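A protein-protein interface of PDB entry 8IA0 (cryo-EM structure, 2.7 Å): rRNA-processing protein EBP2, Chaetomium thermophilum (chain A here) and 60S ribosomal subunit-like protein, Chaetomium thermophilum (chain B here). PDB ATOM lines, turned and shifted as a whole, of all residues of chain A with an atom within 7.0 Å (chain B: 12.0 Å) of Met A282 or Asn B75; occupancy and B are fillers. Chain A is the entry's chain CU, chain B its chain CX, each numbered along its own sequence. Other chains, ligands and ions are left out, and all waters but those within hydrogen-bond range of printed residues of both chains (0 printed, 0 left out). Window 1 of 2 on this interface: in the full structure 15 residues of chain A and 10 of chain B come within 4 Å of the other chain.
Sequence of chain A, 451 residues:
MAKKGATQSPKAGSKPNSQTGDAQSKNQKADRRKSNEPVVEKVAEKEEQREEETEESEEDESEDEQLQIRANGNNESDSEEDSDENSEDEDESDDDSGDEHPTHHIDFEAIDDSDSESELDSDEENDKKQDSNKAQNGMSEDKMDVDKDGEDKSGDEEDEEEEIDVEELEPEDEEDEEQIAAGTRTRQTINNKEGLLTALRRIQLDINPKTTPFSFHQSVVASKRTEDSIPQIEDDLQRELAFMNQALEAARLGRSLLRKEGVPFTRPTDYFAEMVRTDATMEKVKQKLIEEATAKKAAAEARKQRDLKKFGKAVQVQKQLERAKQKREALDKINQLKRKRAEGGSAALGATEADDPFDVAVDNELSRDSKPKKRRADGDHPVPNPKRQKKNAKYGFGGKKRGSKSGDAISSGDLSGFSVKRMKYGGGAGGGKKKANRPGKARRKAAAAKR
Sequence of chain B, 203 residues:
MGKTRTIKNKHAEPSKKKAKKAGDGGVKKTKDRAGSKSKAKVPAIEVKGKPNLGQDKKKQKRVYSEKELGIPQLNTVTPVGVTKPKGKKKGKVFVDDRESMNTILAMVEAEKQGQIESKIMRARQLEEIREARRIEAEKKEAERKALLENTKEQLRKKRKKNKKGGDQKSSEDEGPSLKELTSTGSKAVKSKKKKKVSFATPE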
ATOM      1  N   ARG A 267      22.560  18.760 -10.595  1.00  0.00           N
ATOM      2  CA  ARG A 267      21.712  19.927 -10.403  1.00  0.00           C
ATOM      3  C   ARG A 267      22.164  21.048 -11.327  1.00  0.00           C
ATOM      4  O   ARG A 267      23.320  21.476 -11.244  1.00  0.00           O
ATOM      5  CB  ARG A 267      21.766  20.389  -8.954  1.00  0.00           C
ATOM      6  CG  ARG A 267      20.695  21.392  -8.577  1.00  0.00           C
ATOM      7  CD  ARG A 267      21.091  22.167  -7.335  1.00  0.00           C
ATOM      8  NE  ARG A 267      20.062  23.121  -6.944  1.00  0.00           N
ATOM      9  CZ  ARG A 267      20.219  24.053  -6.016  1.00  0.00           C
ATOM     10  NH1 ARG A 267      21.353  24.181  -5.350  1.00  0.00           N
ATOM     11  NH2 ARG A 267      19.211  24.877  -5.748  1.00  0.00           N
ATOM     12  N   MET A 275      16.267  24.383   0.121  1.00  0.00           N
ATOM     13  CA  MET A 275      17.211  23.423   0.666  1.00  0.00           C
ATOM     14  C   MET A 275      16.729  22.948   2.030  1.00  0.00           C
ATOM     15  O   MET A 275      15.727  23.427   2.565  1.00  0.00           O
ATOM     16  CB  MET A 275      18.612  24.035   0.789  1.00  0.00           C
ATOM     17  CG  MET A 275      19.134  24.700  -0.473  1.00  0.00           C
ATOM     18  SD  MET A 275      20.044  23.578  -1.547  1.00  0.00           S
ATOM     19  CE  MET A 275      18.812  23.249  -2.794  1.00  0.00           C
ATOM     20  N   ARG A 277      18.759  23.242   4.631  1.00  0.00           N
ATOM     21  CA  ARG A 277      19.334  24.258   5.497  1.00  0.00           C
ATOM     22  C   ARG A 277      19.146  25.626   4.859  1.00  0.00           C
ATOM     23  O   ARG A 277      19.446  25.816   3.677  1.00  0.00           O
ATOM     24  CB  ARG A 277      20.818  23.987   5.748  1.00  0.00           C
ATOM     25  CG  ARG A 277      21.070  22.795   6.651  1.00  0.00           C
ATOM     26  CD  ARG A 277      22.376  22.110   6.314  1.00  0.00           C
ATOM     27  NE  ARG A 277      23.531  22.898   6.719  1.00  0.00           N
ATOM     28  CZ  ARG A 277      24.123  22.801   7.901  1.00  0.00           C
ATOM     29  NH1 ARG A 277      23.684  21.965   8.827  1.00  0.00           N
ATOM     30  NH2 ARG A 277      25.184  23.556   8.158  1.00  0.00           N
ATOM     31  N   THR A 278      18.643  26.574   5.644  1.00  0.00           N
ATOM     32  CA  THR A 278      18.271  27.879   5.124  1.00  0.00           C
ATOM     33  C   THR A 278      19.504  28.670   4.694  1.00  0.00           C
ATOM     34  O   THR A 278      20.648  28.300   4.971  1.00  0.00           O
ATOM     35  CB  THR A 278      17.481  28.668   6.165  1.00  0.00           C
ATOM     36  OG1 THR A 278      18.293  28.872   7.327  1.00  0.00           O
ATOM     37  CG2 THR A 278      16.223  27.916   6.561  1.00  0.00           C
ATOM     38  N   ASP A 279      19.252  29.780   3.996  1.00  0.00           N
ATOM     39  CA  ASP A 279      20.339  30.657   3.576  1.00  0.00           C
ATOM     40  C   ASP A 279      21.062  31.248   4.778  1.00  0.00           C
ATOM     41  O   ASP A 279      22.292  31.378   4.772  1.00  0.00           O
ATOM     42  CB  ASP A 279      19.798  31.773   2.682  1.00  0.00           C
ATOM     43  CG  ASP A 279      19.732  31.372   1.226  1.00  0.00           C
ATOM     44  OD1 ASP A 279      19.866  30.166   0.938  1.00  0.00           O
ATOM     45  OD2 ASP A 279      19.550  32.262   0.368  1.00  0.00           O
ATOM     46  N   ALA A 280      20.311  31.623   5.816  1.00  0.00           N
ATOM     47  CA  ALA A 280      20.924  32.182   7.015  1.00  0.00           C
ATOM     48  C   ALA A 280      21.826  31.166   7.701  1.00  0.00           C
ATOM     49  O   ALA A 280      22.904  31.517   8.194  1.00  0.00           O
ATOM     50  CB  ALA A 280      19.841  32.674   7.975  1.00  0.00           C
ATOM     51  N   THR A 281      21.398  29.903   7.749  1.00  0.00           N
ATOM     52  CA  THR A 281      22.218  28.866   8.365  1.00  0.00           C
ATOM     53  C   THR A 281      23.536  28.689   7.624  1.00  0.00           C
ATOM     54  O   THR A 281      24.601  28.608   8.246  1.00  0.00           O
ATOM     55  CB  THR A 281      21.447  27.546   8.407  1.00  0.00           C
ATOM     56  OG1 THR A 281      20.437  27.614   9.419  1.00  0.00           O
ATOM     57  CG2 THR A 281      22.380  26.388   8.712  1.00  0.00           C
ATOM     58  N   MET A 282      23.489  28.643   6.292  1.00  0.00           N
ATOM     59  CA  MET A 282      24.713  28.435   5.528  1.00  0.00           C
ATOM     60  C   MET A 282      25.565  29.695   5.469  1.00  0.00           C
ATOM     61  O   MET A 282      26.772  29.613   5.219  1.00  0.00           O
ATOM     62  CB  MET A 282      24.381  27.942   4.121  1.00  0.00           C
ATOM     63  CG  MET A 282      23.762  26.555   4.096  1.00  0.00           C
ATOM     64  SD  MET A 282      24.926  25.268   4.582  1.00  0.00           S
ATOM     65  CE  MET A 282      25.705  24.881   3.022  1.00  0.00           C
ATOM     66  N   GLU A 283      24.962  30.866   5.682  1.00  0.00           N
ATOM     67  CA  GLU A 283      25.758  32.079   5.827  1.00  0.00           C
ATOM     68  C   GLU A 283      26.528  32.065   7.139  1.00  0.00           C
ATOM     69  O   GLU A 283      27.667  32.539   7.206  1.00  0.00           O
ATOM     70  CB  GLU A 283      24.864  33.315   5.740  1.00  0.00           C
ATOM     71  CG  GLU A 283      25.611  34.586   5.383  1.00  0.00           C
ATOM     72  CD  GLU A 283      25.509  34.932   3.912  1.00  0.00           C
ATOM     73  OE1 GLU A 283      24.445  34.675   3.311  1.00  0.00           O
ATOM     74  OE2 GLU A 283      26.493  35.463   3.354  1.00  0.00           O
ATOM     75  N   LYS A 284      25.917  31.527   8.197  1.00  0.00           N
ATOM     76  CA  LYS A 284      26.632  31.352   9.457  1.00  0.00           C
ATOM     77  C   LYS A 284      27.763  30.344   9.307  1.00  0.00           C
ATOM     78  O   LYS A 284      28.835  30.510   9.898  1.00  0.00           O
ATOM     79  CB  LYS A 284      25.663  30.910  10.551  1.00  0.00           C
ATOM     80  CG  LYS A 284      24.617  31.945  10.922  1.00  0.00           C
ATOM     81  CD  LYS A 284      23.731  31.447  12.051  1.00  0.00           C
ATOM     82  CE  LYS A 284      23.325  32.581  12.971  1.00  0.00           C
ATOM     83  NZ  LYS A 284      23.173  33.865  12.235  1.00  0.00           N
ATOM     84  N   VAL A 285      27.537  29.285   8.528  1.00  0.00           N
ATOM     85  CA  VAL A 285      28.564  28.264   8.332  1.00  0.00           C
ATOM     86  C   VAL A 285      29.756  28.847   7.585  1.00  0.00           C
ATOM     87  O   VAL A 285      30.915  28.592   7.935  1.00  0.00           O
ATOM     88  CB  VAL A 285      27.973  27.047   7.599  1.00  0.00           C
ATOM     89  CG1 VAL A 285      29.075  26.094   7.171  1.00  0.00           C
ATOM     90  CG2 VAL A 285      26.970  26.335   8.486  1.00  0.00           C
ATOM     91  N   LYS A 286      29.493  29.640   6.545  1.00  0.00           N
ATOM     92  CA  LYS A 286      30.584  30.264   5.802  1.00  0.00           C
ATOM     93  C   LYS A 286      31.348  31.255   6.668  1.00  0.00           C
ATOM     94  O   LYS A 286      32.580  31.339   6.588  1.00  0.00           O
ATOM     95  CB  LYS A 286      30.049  30.954   4.549  1.00  0.00           C
ATOM     96  CG  LYS A 286      31.035  30.969   3.393  1.00  0.00           C
ATOM     97  CD  LYS A 286      31.230  32.367   2.833  1.00  0.00           C
ATOM     98  CE  LYS A 286      29.907  33.087   2.658  1.00  0.00           C
ATOM     99  NZ  LYS A 286      30.043  34.292   1.795  1.00  0.00           N
ATOM    100  N   GLN A 287      30.637  32.017   7.502  1.00  0.00           N
ATOM    101  CA  GLN A 287      31.300  33.009   8.342  1.00  0.00           C
ATOM    102  C   GLN A 287      32.253  32.354   9.332  1.00  0.00           C
ATOM    103  O   GLN A 287      33.348  32.872   9.582  1.00  0.00           O
ATOM    104  CB  GLN A 287      30.262  33.855   9.078  1.00  0.00           C
ATOM    105  CG  GLN A 287      29.625  34.933   8.223  1.00  0.00           C
ATOM    106  CD  GLN A 287      30.649  35.819   7.544  1.00  0.00           C
ATOM    107  OE1 GLN A 287      31.595  36.292   8.174  1.00  0.00           O
ATOM    108  NE2 GLN A 287      30.466  36.049   6.249  1.00  0.00           N
ATOM    109  N   GLU B  66      38.129  36.221   0.643  1.00  0.00           N
ATOM    110  CA  GLU B  66      37.797  34.804   0.717  1.00  0.00           C
ATOM    111  C   GLU B  66      38.474  34.000  -0.383  1.00  0.00           C
ATOM    112  O   GLU B  66      38.563  32.773  -0.271  1.00  0.00           O
ATOM    113  CB  GLU B  66      36.282  34.609   0.648  1.00  0.00           C
ATOM    114  CG  GLU B  66      35.488  35.629   1.448  1.00  0.00           C
ATOM    115  CD  GLU B  66      34.008  35.602   1.119  1.00  0.00           C
ATOM    116  OE1 GLU B  66      33.559  34.634   0.470  1.00  0.00           O
ATOM    117  OE2 GLU B  66      33.294  36.547   1.513  1.00  0.00           O
ATOM    118  N   ILE B  71      38.749  28.551   1.367  1.00  0.00           N
ATOM    119  CA  ILE B  71      37.448  28.398   2.009  1.00  0.00           C
ATOM    120  C   ILE B  71      36.595  27.482   1.137  1.00  0.00           C
ATOM    121  O   ILE B  71      36.446  27.756  -0.064  1.00  0.00           O
ATOM    122  CB  ILE B  71      36.772  29.756   2.215  1.00  0.00           C
ATOM    123  CG1 ILE B  71      37.190  30.340   3.559  1.00  0.00           C
ATOM    124  CG2 ILE B  71      35.261  29.619   2.176  1.00  0.00           C
ATOM    125  CD1 ILE B  71      36.769  31.763   3.745  1.00  0.00           C
ATOM    126  N   PRO B  72      36.049  26.394   1.678  1.00  0.00           N
ATOM    127  CA  PRO B  72      35.217  25.502   0.863  1.00  0.00           C
ATOM    128  C   PRO B  72      33.974  26.207   0.346  1.00  0.00           C
ATOM    129  O   PRO B  72      33.396  27.070   1.010  1.00  0.00           O
ATOM    130  CB  PRO B  72      34.850  24.371   1.832  1.00  0.00           C
ATOM    131  CG  PRO B  72      35.867  24.447   2.922  1.00  0.00           C
ATOM    132  CD  PRO B  72      36.220  25.891   3.050  1.00  0.00           C
ATOM    133  N   GLN B  73      33.565  25.827  -0.861  1.00  0.00           N
ATOM    134  CA  GLN B  73      32.354  26.368  -1.460  1.00  0.00           C
ATOM    135  C   GLN B  73      31.124  25.650  -0.920  1.00  0.00           C
ATOM    136  O   GLN B  73      31.128  24.431  -0.734  1.00  0.00           O
ATOM    137  CB  GLN B  73      32.422  26.256  -2.982  1.00  0.00           C
ATOM    138  CG  GLN B  73      33.834  26.361  -3.522  1.00  0.00           C
ATOM    139  CD  GLN B  73      33.906  26.172  -5.018  1.00  0.00           C
ATOM    140  OE1 GLN B  73      33.604  27.084  -5.786  1.00  0.00           O
ATOM    141  NE2 GLN B  73      34.342  24.996  -5.442  1.00  0.00           N
ATOM    142  N   LEU B  74      30.069  26.419  -0.671  1.00  0.00           N
ATOM    143  CA  LEU B  74      28.896  25.944   0.047  1.00  0.00           C
ATOM    144  C   LEU B  74      27.698  25.849  -0.888  1.00  0.00           C
ATOM    145  O   LEU B  74      27.473  26.735  -1.717  1.00  0.00           O
ATOM    146  CB  LEU B  74      28.567  26.874   1.217  1.00  0.00           C
ATOM    147  CG  LEU B  74      29.030  26.432   2.605  1.00  0.00           C
ATOM    148  CD1 LEU B  74      30.445  25.878   2.566  1.00  0.00           C
ATOM    149  CD2 LEU B  74      28.931  27.579   3.592  1.00  0.00           C
ATOM    150  N   ASN B  75      26.923  24.779  -0.736  1.00  0.00           N
ATOM    151  CA  ASN B  75      25.724  24.585  -1.539  1.00  0.00           C
ATOM    152  C   ASN B  75      24.576  25.391  -0.949  1.00  0.00           C
ATOM    153  O   ASN B  75      24.282  25.290   0.245  1.00  0.00           O
ATOM    154  CB  ASN B  75      25.358  23.105  -1.604  1.00  0.00           C
ATOM    155  CG  ASN B  75      24.480  22.775  -2.790  1.00  0.00           C
ATOM    156  OD1 ASN B  75      24.474  23.487  -3.791  1.00  0.00           O
ATOM    157  ND2 ASN B  75      23.734  21.682  -2.687  1.00  0.00           N
ATOM    158  N   THR B  76      23.929  26.192  -1.787  1.00  0.00           N
ATOM    159  CA  THR B  76      22.901  27.122  -1.344  1.00  0.00           C
ATOM    160  C   THR B  76      21.793  27.088  -2.394  1.00  0.00           C
ATOM    161  O   THR B  76      21.771  26.212  -3.265  1.00  0.00           O
ATOM    162  CB  THR B  76      23.534  28.507  -1.128  1.00  0.00           C
ATOM    163  OG1 THR B  76      24.728  28.361  -0.352  1.00  0.00           O
ATOM    164  CG2 THR B  76      22.617  29.430  -0.347  1.00  0.00           C
ATOM    165  N   VAL B  77      20.854  28.034  -2.318  1.00  0.00           N
ATOM    166  CA  VAL B  77      19.844  28.161  -3.364  1.00  0.00           C
ATOM    167  C   VAL B  77      20.514  28.405  -4.710  1.00  0.00           C
ATOM    168  O   VAL B  77      20.024  27.964  -5.756  1.00  0.00           O
ATOM    169  CB  VAL B  77      18.846  29.278  -3.007  1.00  0.00           C
ATOM    170  CG1 VAL B  77      17.803  29.434  -4.095  1.00  0.00           C
ATOM    171  CG2 VAL B  77      18.180  28.983  -1.675  1.00  0.00           C
ATOM    172  N   THR B  78      21.653  29.089  -4.702  1.00  0.00           N
ATOM    173  CA  THR B  78      22.502  29.150  -5.883  1.00  0.00           C
ATOM    174  C   THR B  78      23.337  27.879  -5.958  1.00  0.00           C
ATOM    175  O   THR B  78      24.156  27.637  -5.065  1.00  0.00           O
ATOM    176  CB  THR B  78      23.410  30.368  -5.832  1.00  0.00           C
ATOM    177  OG1 THR B  78      22.721  31.452  -5.198  1.00  0.00           O
ATOM    178  CG2 THR B  78      23.817  30.784  -7.237  1.00  0.00           C
ATOM    179  N   PRO B  79      23.164  27.049  -6.982  1.00  0.00           N
ATOM    180  CA  PRO B  79      23.874  25.767  -7.022  1.00  0.00           C
ATOM    181  C   PRO B  79      25.380  25.944  -7.126  1.00  0.00           C
ATOM    182  O   PRO B  79      25.882  26.854  -7.790  1.00  0.00           O
ATOM    183  CB  PRO B  79      23.313  25.088  -8.276  1.00  0.00           C
ATOM    184  CG  PRO B  79      22.040  25.812  -8.578  1.00  0.00           C
ATOM    185  CD  PRO B  79      22.255  27.214  -8.125  1.00  0.00           C
ATOM    186  N   VAL B  80      26.104  25.048  -6.452  1.00  0.00           N
ATOM    187  CA  VAL B  80      27.555  25.016  -6.595  1.00  0.00           C
ATOM    188  C   VAL B  80      27.945  24.511  -7.974  1.00  0.00           C
ATOM    189  O   VAL B  80      28.948  24.956  -8.545  1.00  0.00           O
ATOM    190  CB  VAL B  80      28.193  24.159  -5.487  1.00  0.00           C
ATOM    191  CG1 VAL B  80      28.343  24.966  -4.214  1.00  0.00           C
ATOM    192  CG2 VAL B  80      27.366  22.913  -5.237  1.00  0.00           C
ATOM    193  N   GLY B  81      27.175  23.583  -8.529  1.00  0.00           N
ATOM    194  CA  GLY B  81      27.528  23.000  -9.803  1.00  0.00           C
ATOM    195  C   GLY B  81      28.717  22.063  -9.670  1.00  0.00           C
ATOM    196  O   GLY B  81      29.072  21.599  -8.584  1.00  0.00           O
ATOM    197  N   VAL B  82      29.340  21.785 -10.812  1.00  0.00           N
ATOM    198  CA  VAL B  82      30.530  20.943 -10.848  1.00  0.00           C
ATOM    199  C   VAL B  82      31.725  21.815 -10.485  1.00  0.00           C
ATOM    200  O   VAL B  82      32.068  22.751 -11.210  1.00  0.00           O
ATOM    201  CB  VAL B  82      30.715  20.286 -12.219  1.00  0.00           C
ATOM    202  CG1 VAL B  82      31.587  19.049 -12.095  1.00  0.00           C
ATOM    203  CG2 VAL B  82      29.367  19.931 -12.820  1.00  0.00           C
ATOM    204  N   THR B  83      32.357  21.511  -9.358  1.00  0.00           N
ATOM    205  CA  THR B  83      33.473  22.301  -8.873  1.00  0.00           C
ATOM    206  C   THR B  83      34.783  21.791  -9.467  1.00  0.00           C
ATOM    207  O   THR B  83      34.900  20.637  -9.886  1.00  0.00           O
ATOM    208  CB  THR B  83      33.532  22.258  -7.349  1.00  0.00           C
ATOM    209  OG1 THR B  83      33.545  20.896  -6.912  1.00  0.00           O
ATOM    210  CG2 THR B  83      32.304  22.937  -6.766  1.00  0.00           C
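Among the printed residues, merely in contact across the chains: Asp A279 with Thr B76, Met A282 with Asn B75, Asp A279 with Val B77, Met A282 with Leu B74, Arg A267 with Pro B79, Arg A267 with Asn B75, Lys A286 with Leu B74 and Val A285 with Leu B74.
Hydrophobic or aromatic side chains of chain A that line the printed part of chain B: Met A275, Met A282 and Val A285.
Printed residues of chain B that touch a printed residue of chain A: Glu B66, Leu B74, Asn B75, Thr B76, Val B77 and Pro B79.
Hydrophobic or aromatic side chains of chain B that line the printed part of chain A: Leu B74, Val B77 and Pro B79.
Along chain B the printed residues that touch a printed residue of chain A span positions 66 to 79.
Among the printed residues, Asp or Glu carboxylates within 4 Å of a Lys or Arg side-chain nitrogen of the other chain: Lys A286 with Glu B66 (3.8 Å).
Of the printed residues of chain B, Arg A267 touches Asn B75, Thr B76, Val B77 and Pro B79.
No residue of chain B comes within 4 Å of Arg A277.
No residue of chain B comes within 4 Å of Thr A278.
Of chain B, only Thr B76 and Val B77 come within 4 Å of Asp A279.
No residue of chain B comes within 4 Å of Ala A280.
No residue of chain B comes within 4 Å of Thr A281.
Of the printed residues of chain B, Met A282 touches Leu B74 (3.4 Å) and Asn B75 (3.1 Å).
Lys A284 touches none of the printed residues of chain B.
Val A285 touches just one residue of chain B: Leu B74.
Printed residues of chain B within 4 Å of Lys A286: Glu B66 (3.8 Å) and Leu B74 (3.6 Å).
Asn B75 touches just these residues of chain A: Arg A267 (3.6 Å) and Met A282 (3.1 Å).
Of the printed residues of chain A, Thr B76 touches Arg A267 (2.9 Å), Met A275 (3.6 Å) and Asp A279 (3.1 Å).
Of the printed residues of chain A, Pro B79 touches Arg A267 (3.4 Å).
Val B80 touches none of the printed residues of chain A.
The nearest residue of chain B that does not touch Met A282 is Thr B76 (4.5 Å).
The nearest printed residue of chain A that does not touch Leu B74 is Glu A283 (5.6 Å).
The guanidinium group (NE) of Arg A277 lies within hydrogen-bond range of the side-chain sulfur (SD) of Met A282, 3.5 Å away.
OG1 of Thr B76 sits at hydrogen-bond distance from O of Leu B74, 3.5 Å away.
The side-chain amide oxygen (OD1) of Asn B75 lies close to the backbone NH (N) of Val B80 (3.5 Å).
The backbone carbonyl oxygen of Thr B76 lies within hydrogen-bond range of the guanidinium group of Arg A267 (2.9 Å).
NH2 of Arg A267 is in hydrogen-bond range of O of Val B77, 3.2 Å away.
NZ of Lys A286 lies within salt-bridge range of OE1 of Glu B66, at 3.8 Å.
The side-chain sulfur of Met A275 lies close to the backbone carbonyl oxygen of Thr B76.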
